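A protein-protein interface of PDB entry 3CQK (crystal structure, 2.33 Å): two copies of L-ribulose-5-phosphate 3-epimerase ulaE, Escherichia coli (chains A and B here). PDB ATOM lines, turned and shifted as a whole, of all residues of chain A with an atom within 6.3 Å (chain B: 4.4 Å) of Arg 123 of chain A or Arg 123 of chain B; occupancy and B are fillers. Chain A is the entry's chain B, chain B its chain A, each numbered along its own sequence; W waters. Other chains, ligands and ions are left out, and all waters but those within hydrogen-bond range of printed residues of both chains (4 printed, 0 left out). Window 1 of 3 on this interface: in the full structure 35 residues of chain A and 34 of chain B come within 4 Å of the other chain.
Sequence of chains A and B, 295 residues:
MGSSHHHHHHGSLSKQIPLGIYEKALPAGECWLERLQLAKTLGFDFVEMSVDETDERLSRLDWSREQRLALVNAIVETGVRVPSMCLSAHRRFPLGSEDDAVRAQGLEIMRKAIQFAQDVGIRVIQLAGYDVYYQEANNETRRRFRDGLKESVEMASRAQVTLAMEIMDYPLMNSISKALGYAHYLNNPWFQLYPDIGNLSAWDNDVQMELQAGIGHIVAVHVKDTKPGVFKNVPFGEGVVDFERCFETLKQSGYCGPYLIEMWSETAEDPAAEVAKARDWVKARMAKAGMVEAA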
ATOM      1  N   VAL A  82     -16.211 -31.205  -1.853  1.00  0.00           N
ATOM      2  CA  VAL A  82     -15.213 -30.193  -2.189  1.00  0.00           C
ATOM      3  C   VAL A  82     -16.006 -29.015  -2.747  1.00  0.00           C
ATOM      4  O   VAL A  82     -16.070 -28.834  -3.958  1.00  0.00           O
ATOM      5  CB  VAL A  82     -14.095 -30.711  -3.186  1.00  0.00           C
ATOM      6  CG1 VAL A  82     -13.051 -29.634  -3.444  1.00  0.00           C
ATOM      7  CG2 VAL A  82     -13.411 -31.983  -2.654  1.00  0.00           C
ATOM      8  N   PRO A  83     -16.644 -28.226  -1.856  1.00  0.00           N
ATOM      9  CA  PRO A  83     -17.582 -27.189  -2.281  1.00  0.00           C
ATOM     10  C   PRO A  83     -16.923 -25.886  -2.740  1.00  0.00           C
ATOM     11  O   PRO A  83     -17.572 -25.072  -3.394  1.00  0.00           O
ATOM     12  CB  PRO A  83     -18.416 -26.943  -1.023  1.00  0.00           C
ATOM     13  CG  PRO A  83     -17.474 -27.177   0.083  1.00  0.00           C
ATOM     14  CD  PRO A  83     -16.535 -28.280  -0.387  1.00  0.00           C
ATOM     15  N   SER A  84     -15.652 -25.694  -2.409  1.00  0.00           N
ATOM     16  CA  SER A  84     -14.981 -24.460  -2.755  1.00  0.00           C
ATOM     17  C   SER A  84     -13.558 -24.666  -3.280  1.00  0.00           C
ATOM     18  O   SER A  84     -12.923 -25.696  -3.021  1.00  0.00           O
ATOM     19  CB  SER A  84     -15.019 -23.471  -1.580  1.00  0.00           C
ATOM     20  OG  SER A  84     -14.706 -24.095  -0.340  1.00  0.00           O
ATOM     21  N   MET A  85     -13.098 -23.686  -4.051  1.00  0.00           N
ATOM     22  CA  MET A  85     -11.753 -23.642  -4.560  1.00  0.00           C
ATOM     23  C   MET A  85     -11.061 -22.318  -4.219  1.00  0.00           C
ATOM     24  O   MET A  85     -11.536 -21.261  -4.614  1.00  0.00           O
ATOM     25  CB  MET A  85     -11.800 -23.766  -6.071  1.00  0.00           C
ATOM     26  CG  MET A  85     -10.439 -23.779  -6.716  1.00  0.00           C
ATOM     27  SD  MET A  85     -10.472 -23.312  -8.472  1.00  0.00           S
ATOM     28  CE  MET A  85     -11.575 -24.583  -9.136  1.00  0.00           C
ATOM     29  N   ALA A 117     -14.822 -26.039 -12.035  1.00  0.00           N
ATOM     30  CA  ALA A 117     -15.918 -25.984 -11.063  1.00  0.00           C
ATOM     31  C   ALA A 117     -17.242 -26.605 -11.577  1.00  0.00           C
ATOM     32  O   ALA A 117     -17.922 -27.328 -10.822  1.00  0.00           O
ATOM     33  CB  ALA A 117     -16.145 -24.553 -10.591  1.00  0.00           C
ATOM     34  N   GLN A 118     -17.599 -26.317 -12.839  1.00  0.00           N
ATOM     35  CA  GLN A 118     -18.758 -26.953 -13.519  1.00  0.00           C
ATOM     36  C   GLN A 118     -18.632 -28.489 -13.567  1.00  0.00           C
ATOM     37  O   GLN A 118     -19.522 -29.208 -13.084  1.00  0.00           O
ATOM     38  CB  GLN A 118     -18.929 -26.435 -14.961  1.00  0.00           C
ATOM     39  CG  GLN A 118     -19.491 -25.006 -15.119  1.00  0.00           C
ATOM     40  CD  GLN A 118     -19.480 -24.509 -16.579  1.00  0.00           C
ATOM     41  OE1 GLN A 118     -18.419 -24.271 -17.157  1.00  0.00           O
ATOM     42  NE2 GLN A 118     -20.668 -24.319 -17.160  1.00  0.00           N
ATOM     43  N   VAL A 120     -16.694 -30.594 -11.958  1.00  0.00           N
ATOM     44  CA  VAL A 120     -16.512 -31.286 -10.681  1.00  0.00           C
ATOM     45  C   VAL A 120     -17.512 -30.925  -9.588  1.00  0.00           C
ATOM     46  O   VAL A 120     -17.555 -31.597  -8.554  1.00  0.00           O
ATOM     47  CB  VAL A 120     -15.061 -31.139 -10.155  1.00  0.00           C
ATOM     48  CG1 VAL A 120     -14.976 -31.591  -8.724  1.00  0.00           C
ATOM     49  CG2 VAL A 120     -14.125 -31.996 -10.995  1.00  0.00           C
ATOM     50  N   GLY A 121     -18.324 -29.889  -9.811  1.00  0.00           N
ATOM     51  CA  GLY A 121     -19.399 -29.574  -8.878  1.00  0.00           C
ATOM     52  C   GLY A 121     -18.925 -28.696  -7.718  1.00  0.00           C
ATOM     53  O   GLY A 121     -19.468 -28.755  -6.595  1.00  0.00           O
ATOM     54  N   ILE A 122     -17.910 -27.880  -7.981  1.00  0.00           N
ATOM     55  CA  ILE A 122     -17.461 -26.922  -6.973  1.00  0.00           C
ATOM     56  C   ILE A 122     -18.477 -25.775  -6.904  1.00  0.00           C
ATOM     57  O   ILE A 122     -18.906 -25.271  -7.937  1.00  0.00           O
ATOM     58  CB  ILE A 122     -16.037 -26.430  -7.272  1.00  0.00           C
ATOM     59  CG1 ILE A 122     -15.050 -27.588  -7.034  1.00  0.00           C
ATOM     60  CG2 ILE A 122     -15.688 -25.218  -6.424  1.00  0.00           C
ATOM     61  CD1 ILE A 122     -13.571 -27.245  -7.306  1.00  0.00           C
ATOM     62  N   ARG A 123     -18.877 -25.386  -5.693  1.00  0.00           N
ATOM     63  CA  ARG A 123     -19.924 -24.368  -5.510  1.00  0.00           C
ATOM     64  C   ARG A 123     -19.404 -22.955  -5.653  1.00  0.00           C
ATOM     65  O   ARG A 123     -20.029 -22.133  -6.344  1.00  0.00           O
ATOM     66  CB  ARG A 123     -20.649 -24.508  -4.156  1.00  0.00           C
ATOM     67  CG  ARG A 123     -21.096 -25.937  -3.789  1.00  0.00           C
ATOM     68  CD  ARG A 123     -21.886 -26.627  -4.890  1.00  0.00           C
ATOM     69  NE  ARG A 123     -23.035 -25.857  -5.352  1.00  0.00           N
ATOM     70  CZ  ARG A 123     -23.918 -26.294  -6.256  1.00  0.00           C
ATOM     71  NH1 ARG A 123     -23.811 -27.516  -6.806  1.00  0.00           N
ATOM     72  NH2 ARG A 123     -24.912 -25.502  -6.620  1.00  0.00           N
ATOM     73  N   VAL A 124     -18.270 -22.679  -5.011  1.00  0.00           N
ATOM     74  CA  VAL A 124     -17.725 -21.327  -4.912  1.00  0.00           C
ATOM     75  C   VAL A 124     -16.254 -21.286  -5.293  1.00  0.00           C
ATOM     76  O   VAL A 124     -15.444 -22.062  -4.774  1.00  0.00           O
ATOM     77  CB  VAL A 124     -17.873 -20.749  -3.472  1.00  0.00           C
ATOM     78  CG1 VAL A 124     -17.172 -19.403  -3.339  1.00  0.00           C
ATOM     79  CG2 VAL A 124     -19.320 -20.612  -3.092  1.00  0.00           C
ATOM     80  N   ILE A 125     -15.902 -20.374  -6.190  1.00  0.00           N
ATOM     81  CA  ILE A 125     -14.495 -20.089  -6.414  1.00  0.00           C
ATOM     82  C   ILE A 125     -14.088 -18.835  -5.639  1.00  0.00           C
ATOM     83  O   ILE A 125     -14.612 -17.753  -5.881  1.00  0.00           O
ATOM     84  CB  ILE A 125     -14.138 -19.930  -7.888  1.00  0.00           C
ATOM     85  CG1 ILE A 125     -14.536 -21.185  -8.665  1.00  0.00           C
ATOM     86  CG2 ILE A 125     -12.649 -19.635  -8.020  1.00  0.00           C
ATOM     87  CD1 ILE A 125     -14.325 -21.083 -10.144  1.00  0.00           C
ATOM     88  N   ALA A 159     -22.069 -19.705 -16.686  1.00  0.00           N
ATOM     89  CA  ALA A 159     -21.842 -21.033 -16.141  1.00  0.00           C
ATOM     90  C   ALA A 159     -22.670 -21.241 -14.885  1.00  0.00           C
ATOM     91  O   ALA A 159     -22.876 -22.377 -14.454  1.00  0.00           O
ATOM     92  CB  ALA A 159     -20.373 -21.236 -15.840  1.00  0.00           C
ATOM     93  N   GLN A 160     -23.127 -20.134 -14.297  1.00  0.00           N
ATOM     94  CA  GLN A 160     -23.839 -20.134 -13.015  1.00  0.00           C
ATOM     95  C   GLN A 160     -22.965 -20.679 -11.887  1.00  0.00           C
ATOM     96  O   GLN A 160     -23.347 -21.602 -11.165  1.00  0.00           O
ATOM     97  CB  GLN A 160     -25.176 -20.879 -13.125  1.00  0.00           C
ATOM     98  CG  GLN A 160     -26.213 -20.174 -13.989  1.00  0.00           C
ATOM     99  CD  GLN A 160     -27.466 -21.012 -14.207  1.00  0.00           C
ATOM    100  OE1 GLN A 160     -27.384 -22.219 -14.492  1.00  0.00           O
ATOM    101  NE2 GLN A 160     -28.632 -20.378 -14.100  1.00  0.00           N
ATOM    102  N   VAL A 161     -21.780 -20.086 -11.747  1.00  0.00           N
ATOM    103  CA  VAL A 161     -20.794 -20.469 -10.739  1.00  0.00           C
ATOM    104  C   VAL A 161     -20.504 -19.230  -9.919  1.00  0.00           C
ATOM    105  O   VAL A 161     -20.270 -18.159 -10.470  1.00  0.00           O
ATOM    106  CB  VAL A 161     -19.445 -21.016 -11.390  1.00  0.00           C
ATOM    107  CG1 VAL A 161     -18.346 -21.282 -10.325  1.00  0.00           C
ATOM    108  CG2 VAL A 161     -19.668 -22.298 -12.218  1.00  0.00           C
ATOM    109  N   THR A 162     -20.515 -19.381  -8.599  1.00  0.00           N
ATOM    110  CA  THR A 162     -20.274 -18.281  -7.659  1.00  0.00           C
ATOM    111  C   THR A 162     -18.781 -17.991  -7.505  1.00  0.00           C
ATOM    112  O   THR A 162     -18.000 -18.879  -7.201  1.00  0.00           O
ATOM    113  CB  THR A 162     -20.844 -18.612  -6.276  1.00  0.00           C
ATOM    114  OG1 THR A 162     -22.231 -18.894  -6.417  1.00  0.00           O
ATOM    115  CG2 THR A 162     -20.691 -17.448  -5.319  1.00  0.00           C
ATOM    116  N   LEU A 163     -18.417 -16.743  -7.720  1.00  0.00           N
ATOM    117  CA  LEU A 163     -17.083 -16.245  -7.434  1.00  0.00           C
ATOM    118  C   LEU A 163     -17.188 -15.409  -6.159  1.00  0.00           C
ATOM    119  O   LEU A 163     -18.022 -14.510  -6.072  1.00  0.00           O
ATOM    120  CB  LEU A 163     -16.565 -15.383  -8.609  1.00  0.00           C
ATOM    121  CG  LEU A 163     -16.568 -16.011 -10.004  1.00  0.00           C
ATOM    122  CD1 LEU A 163     -16.083 -15.020 -11.042  1.00  0.00           C
ATOM    123  CD2 LEU A 163     -15.720 -17.287 -10.022  1.00  0.00           C
ATOM    124  N   TRP A 190     -23.721 -13.632  -8.943  1.00  0.00           N
ATOM    125  CA  TRP A 190     -22.625 -14.598  -8.928  1.00  0.00           C
ATOM    126  C   TRP A 190     -21.335 -14.044  -8.323  1.00  0.00           C
ATOM    127  O   TRP A 190     -20.371 -14.780  -8.146  1.00  0.00           O
ATOM    128  CB  TRP A 190     -22.406 -15.230 -10.318  1.00  0.00           C
ATOM    129  CG  TRP A 190     -23.669 -15.900 -10.800  1.00  0.00           C
ATOM    130  CD1 TRP A 190     -24.530 -15.443 -11.755  1.00  0.00           C
ATOM    131  CD2 TRP A 190     -24.250 -17.093 -10.276  1.00  0.00           C
ATOM    132  NE1 TRP A 190     -25.604 -16.292 -11.873  1.00  0.00           N
ATOM    133  CE2 TRP A 190     -25.452 -17.320 -10.982  1.00  0.00           C
ATOM    134  CE3 TRP A 190     -23.861 -18.011  -9.282  1.00  0.00           C
ATOM    135  CZ2 TRP A 190     -26.276 -18.428 -10.723  1.00  0.00           C
ATOM    136  CZ3 TRP A 190     -24.671 -19.083  -9.016  1.00  0.00           C
ATOM    137  CH2 TRP A 190     -25.874 -19.284  -9.732  1.00  0.00           C
ATOM    138  N   PRO B  83     -27.544 -27.622 -15.522  1.00  0.00           N
ATOM    139  CA  PRO B  83     -27.230 -26.625 -14.499  1.00  0.00           C
ATOM    140  C   PRO B  83     -28.394 -26.316 -13.555  1.00  0.00           C
ATOM    141  O   PRO B  83     -28.185 -25.674 -12.529  1.00  0.00           O
ATOM    142  CB  PRO B  83     -26.915 -25.379 -15.325  1.00  0.00           C
ATOM    143  CG  PRO B  83     -27.746 -25.498 -16.532  1.00  0.00           C
ATOM    144  CD  PRO B  83     -27.795 -26.990 -16.841  1.00  0.00           C
ATOM    145  N   ALA B 117     -28.607 -31.986  -5.926  1.00  0.00           N
ATOM    146  CA  ALA B 117     -27.900 -30.884  -6.566  1.00  0.00           C
ATOM    147  C   ALA B 117     -26.410 -30.929  -6.249  1.00  0.00           C
ATOM    148  O   ALA B 117     -25.582 -30.761  -7.149  1.00  0.00           O
ATOM    149  CB  ALA B 117     -28.503 -29.530  -6.148  1.00  0.00           C
ATOM    150  N   GLY B 121     -24.007 -31.745  -9.301  1.00  0.00           N
ATOM    151  CA  GLY B 121     -23.451 -30.464  -9.706  1.00  0.00           C
ATOM    152  C   GLY B 121     -24.427 -29.554 -10.416  1.00  0.00           C
ATOM    153  O   GLY B 121     -24.042 -28.786 -11.287  1.00  0.00           O
ATOM    154  N   ILE B 122     -25.700 -29.658 -10.048  1.00  0.00           N
ATOM    155  CA  ILE B 122     -26.733 -28.738 -10.494  1.00  0.00           C
ATOM    156  C   ILE B 122     -26.494 -27.387  -9.834  1.00  0.00           C
ATOM    157  O   ILE B 122     -26.304 -27.312  -8.603  1.00  0.00           O
ATOM    158  CB  ILE B 122     -28.147 -29.297 -10.141  1.00  0.00           C
ATOM    159  CG1 ILE B 122     -28.525 -30.443 -11.098  1.00  0.00           C
ATOM    160  CG2 ILE B 122     -29.192 -28.208 -10.177  1.00  0.00           C
ATOM    161  CD1 ILE B 122     -29.836 -31.193 -10.710  1.00  0.00           C
ATOM    162  N   ARG B 123     -26.487 -26.320 -10.640  1.00  0.00           N
ATOM    163  CA  ARG B 123     -26.119 -24.979 -10.136  1.00  0.00           C
ATOM    164  C   ARG B 123     -27.249 -24.261  -9.396  1.00  0.00           C
ATOM    165  O   ARG B 123     -26.997 -23.567  -8.397  1.00  0.00           O
ATOM    166  CB  ARG B 123     -25.571 -24.094 -11.261  1.00  0.00           C
ATOM    167  CG  ARG B 123     -24.539 -24.783 -12.180  1.00  0.00           C
ATOM    168  CD  ARG B 123     -23.275 -25.260 -11.448  1.00  0.00           C
ATOM    169  NE  ARG B 123     -22.744 -24.333 -10.425  1.00  0.00           N
ATOM    170  CZ  ARG B 123     -21.643 -24.605  -9.727  1.00  0.00           C
ATOM    171  NH1 ARG B 123     -21.197 -23.779  -8.804  1.00  0.00           N
ATOM    172  NH2 ARG B 123     -20.987 -25.737  -9.958  1.00  0.00           N
ATOM    173  N   VAL B 124     -28.479 -24.468  -9.881  1.00  0.00           N
ATOM    174  CA  VAL B 124     -29.662 -23.734  -9.455  1.00  0.00           C
ATOM    175  C   VAL B 124     -30.886 -24.652  -9.309  1.00  0.00           C
ATOM    176  O   VAL B 124     -31.202 -25.420 -10.209  1.00  0.00           O
ATOM    177  CB  VAL B 124     -29.952 -22.534 -10.448  1.00  0.00           C
ATOM    178  CG1 VAL B 124     -31.301 -21.908 -10.195  1.00  0.00           C
ATOM    179  CG2 VAL B 124     -28.858 -21.436 -10.345  1.00  0.00           C
ATOM    180  N   ALA B 159     -25.166 -25.912   2.158  1.00  0.00           N
ATOM    181  CA  ALA B 159     -24.726 -26.681   0.994  1.00  0.00           C
ATOM    182  C   ALA B 159     -24.077 -25.791  -0.065  1.00  0.00           C
ATOM    183  O   ALA B 159     -23.400 -26.288  -0.964  1.00  0.00           O
ATOM    184  CB  ALA B 159     -25.924 -27.445   0.379  1.00  0.00           C
ATOM    185  N   GLN B 160     -24.307 -24.482   0.034  1.00  0.00           N
ATOM    186  CA  GLN B 160     -23.860 -23.540  -0.971  1.00  0.00           C
ATOM    187  C   GLN B 160     -24.488 -23.836  -2.341  1.00  0.00           C
ATOM    188  O   GLN B 160     -23.803 -23.874  -3.364  1.00  0.00           O
ATOM    189  CB  GLN B 160     -22.332 -23.497  -1.014  1.00  0.00           C
ATOM    190  CG  GLN B 160     -21.731 -22.847   0.203  1.00  0.00           C
ATOM    191  CD  GLN B 160     -20.213 -22.982   0.276  1.00  0.00           C
ATOM    192  OE1 GLN B 160     -19.655 -24.059   0.054  1.00  0.00           O
ATOM    193  NE2 GLN B 160     -19.545 -21.896   0.628  1.00  0.00           N
ATOM    194  N   VAL B 161     -25.800 -24.043  -2.327  1.00  0.00           N
ATOM    195  CA  VAL B 161     -26.623 -24.327  -3.504  1.00  0.00           C
ATOM    196  C   VAL B 161     -27.633 -23.194  -3.668  1.00  0.00           C
ATOM    197  O   VAL B 161     -28.258 -22.792  -2.713  1.00  0.00           O
ATOM    198  CB  VAL B 161     -27.390 -25.690  -3.357  1.00  0.00           C
ATOM    199  CG1 VAL B 161     -28.426 -25.898  -4.492  1.00  0.00           C
ATOM    200  CG2 VAL B 161     -26.411 -26.867  -3.343  1.00  0.00           C
ATOM    201  N   THR B 162     -27.762 -22.680  -4.886  1.00  0.00           N
ATOM    202  CA  THR B 162     -28.679 -21.589  -5.207  1.00  0.00           C
ATOM    203  C   THR B 162     -30.115 -22.085  -5.367  1.00  0.00           C
ATOM    204  O   THR B 162     -30.397 -23.020  -6.153  1.00  0.00           O
ATOM    205  CB  THR B 162     -28.203 -20.853  -6.493  1.00  0.00           C
ATOM    206  OG1 THR B 162     -26.886 -20.362  -6.278  1.00  0.00           O
ATOM    207  CG2 THR B 162     -29.097 -19.664  -6.881  1.00  0.00           C
HETATM  208  O   HOH W   1     -22.535 -21.850  -7.337  1.00  0.00           O
HETATM  209  O   HOH W   2     -21.384 -27.985 -11.533  1.00  0.00           O
HETATM  210  O   HOH W   3     -17.088 -23.453   1.165  1.00  0.00           O
HETATM  211  O   HOH W   4     -25.012 -22.668  -6.812  1.00  0.00           O
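The backbone carbonyl oxygen of Ile 122 of chain B lies within hydrogen-bond range of the guanidinium group of Arg 123 of chain A (3.0 Å). The guanidinium group (NH1) of Arg 123 of chain B lies within hydrogen-bond range of the backbone carbonyl oxygen (O) of Ile 122 of chain A. O of Arg 123 of chain A is in hydrogen-bond range of NH1 of Arg 123 of chain B (3.2 Å). NE of Arg 123 of chain B sits at hydrogen-bond distance from O of Gln 160 of chain A, 2.9 Å away. NE of Arg 123 of chain A sits at hydrogen-bond distance from O of Gln 160 of chain B (2.9 Å).
Of chain B, only Ala 117, Ile 122, Arg 123, Ala 159, Gln 160 and Val 161 come within 4 Å of Arg 123 of chain A. Arg 123 of chain B touches six residues of chain A. Of the printed residues of chain A, Ile 122 of chain B touches Arg 123 (3.0 Å). Printed residues of chain A within 4 Å of Pro 83 of chain B: Gln 160. Val 82 of chain A touches none of the printed residues of chain B. Gly 121 of chain A touches none of the printed residues of chain B. The nearest residue of chain B that does not touch Arg 123 of chain A is Gly 121 of chain B (4.2 Å). The nearest printed residue of chain B that does not touch Ile 122 of chain A is Gly 121 of chain B (6.4 Å).
Water W4 lies within hydrogen-bond range of the backbone carbonyl oxygen of Arg 123 of chain B (2.7 Å), the guanidinium group of Arg 123 of chain A (2.8 Å) and the side-chain hydroxyl of Thr 162 of chain B (3.0 Å). Water W1 lies within hydrogen-bond range of O of Arg 123 of chain A (2.7 Å), NH1 of Arg 123 of chain B (2.8 Å) and OG1 of Thr 162 of chain A (3.1 Å). Water W2 lies within hydrogen-bond range of the backbone carbonyl oxygen (O) of Gln 118 of chain A (2.7 Å), the guanidinium group (NH2) of Arg 123 of chain B (2.8 Å) and the backbone carbonyl oxygen (O) of Gly 121 of chain B (2.8 Å). Water W3 bridges OE1 of Gln 160 of chain B (2.9 Å) and OG of Ser 84 of chain A (2.9 Å).
Pro 83 of chain A touches Gln 160 of chain B, and with the chains exchanged Gln 160 of chain A touches Pro 83 of chain B. Ala 117 of chain A touches Arg 123 of chain B, and with the chains exchanged Arg 123 of chain A touches Ala 117 of chain B. Arg 123 of chain A touches its own counterpart, Arg 123 of chain B. Arg 123 of chain A touches Ala 159 of chain B, and with the chains exchanged Ala 159 of chain A touches Arg 123 of chain B. Of the 17 pairs that touch across the chains among the printed residues, 15 have their exchanged pair printed and touching as well.
CB of Pro 83 of chain A touches OE1 of Gln 160 of chain B (3.3 Å). Ala 117 of chain A touches Arg 123 of chain B. O of Ala 117 of chain B touches NH1 of Arg 123 of chain A (3.7 Å). O of Ala 159 of chain B touches CG of Arg 123 of chain A, 3.7 Å away. Arg 123 of chain A touches Val 161 of chain B. Val 124 of chain A touches Gln 160 of chain B (CG2 to NE2, 3.9 Å). Pro 83 of chain B touches Gln 160 of chain A (CB to OE1, 3.3 Å). CG2 of Val 124 of chain B touches NE2 of Gln 160 of chain A, at 3.9 Å. CH2 of Trp 190 of chain A touches CG2 of Val 124 of chain B, 3.7 Å away. OG1 of Thr 162 of chain B touches CZ3 of Trp 190 of chain A (3.7 Å).
Of the 10 printed residues of chain B, 9 touch a printed residue of chain A. Hydrophobic or aromatic side chains of chain B within 4 Å of the printed part of chain A: Pro 83, Val 124 and Val 161. Printed residues of chain A that touch a printed residue of chain B: Pro 83, Ala 117, Ile 122, Arg 123, Val 124, Ala 159, Gln 160, Val 161 and Trp 190. Among the printed residues, 17 pairs touch across the chains.
The backbone carbonyl oxygen (O) of Pro 83 of chain B lies within hydrogen-bond range of the backbone NH (N) of Arg 123 of chain B (2.6 Å). N of Val 124 of chain B is in hydrogen-bond range of O of Pro 83 of chain B, 2.9 Å away. The backbone carbonyl oxygen (O) of Pro 83 of chain A sits at hydrogen-bond distance from the backbone NH (N) of Val 124 of chain A, at 3.0 Å. The backbone NH (N) of Met 85 of chain A lies within hydrogen-bond range of the backbone carbonyl oxygen (O) of Val 124 of chain A (2.9 Å). The backbone carbonyl oxygen of Ala 117 of chain A is in hydrogen-bond range of the backbone NH of Ile 122 of chain A (2.9 Å). The backbone NH (N) of Leu 163 of chain A is in hydrogen-bond range of the backbone carbonyl oxygen (O) of Trp 190 of chain A (2.8 Å).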
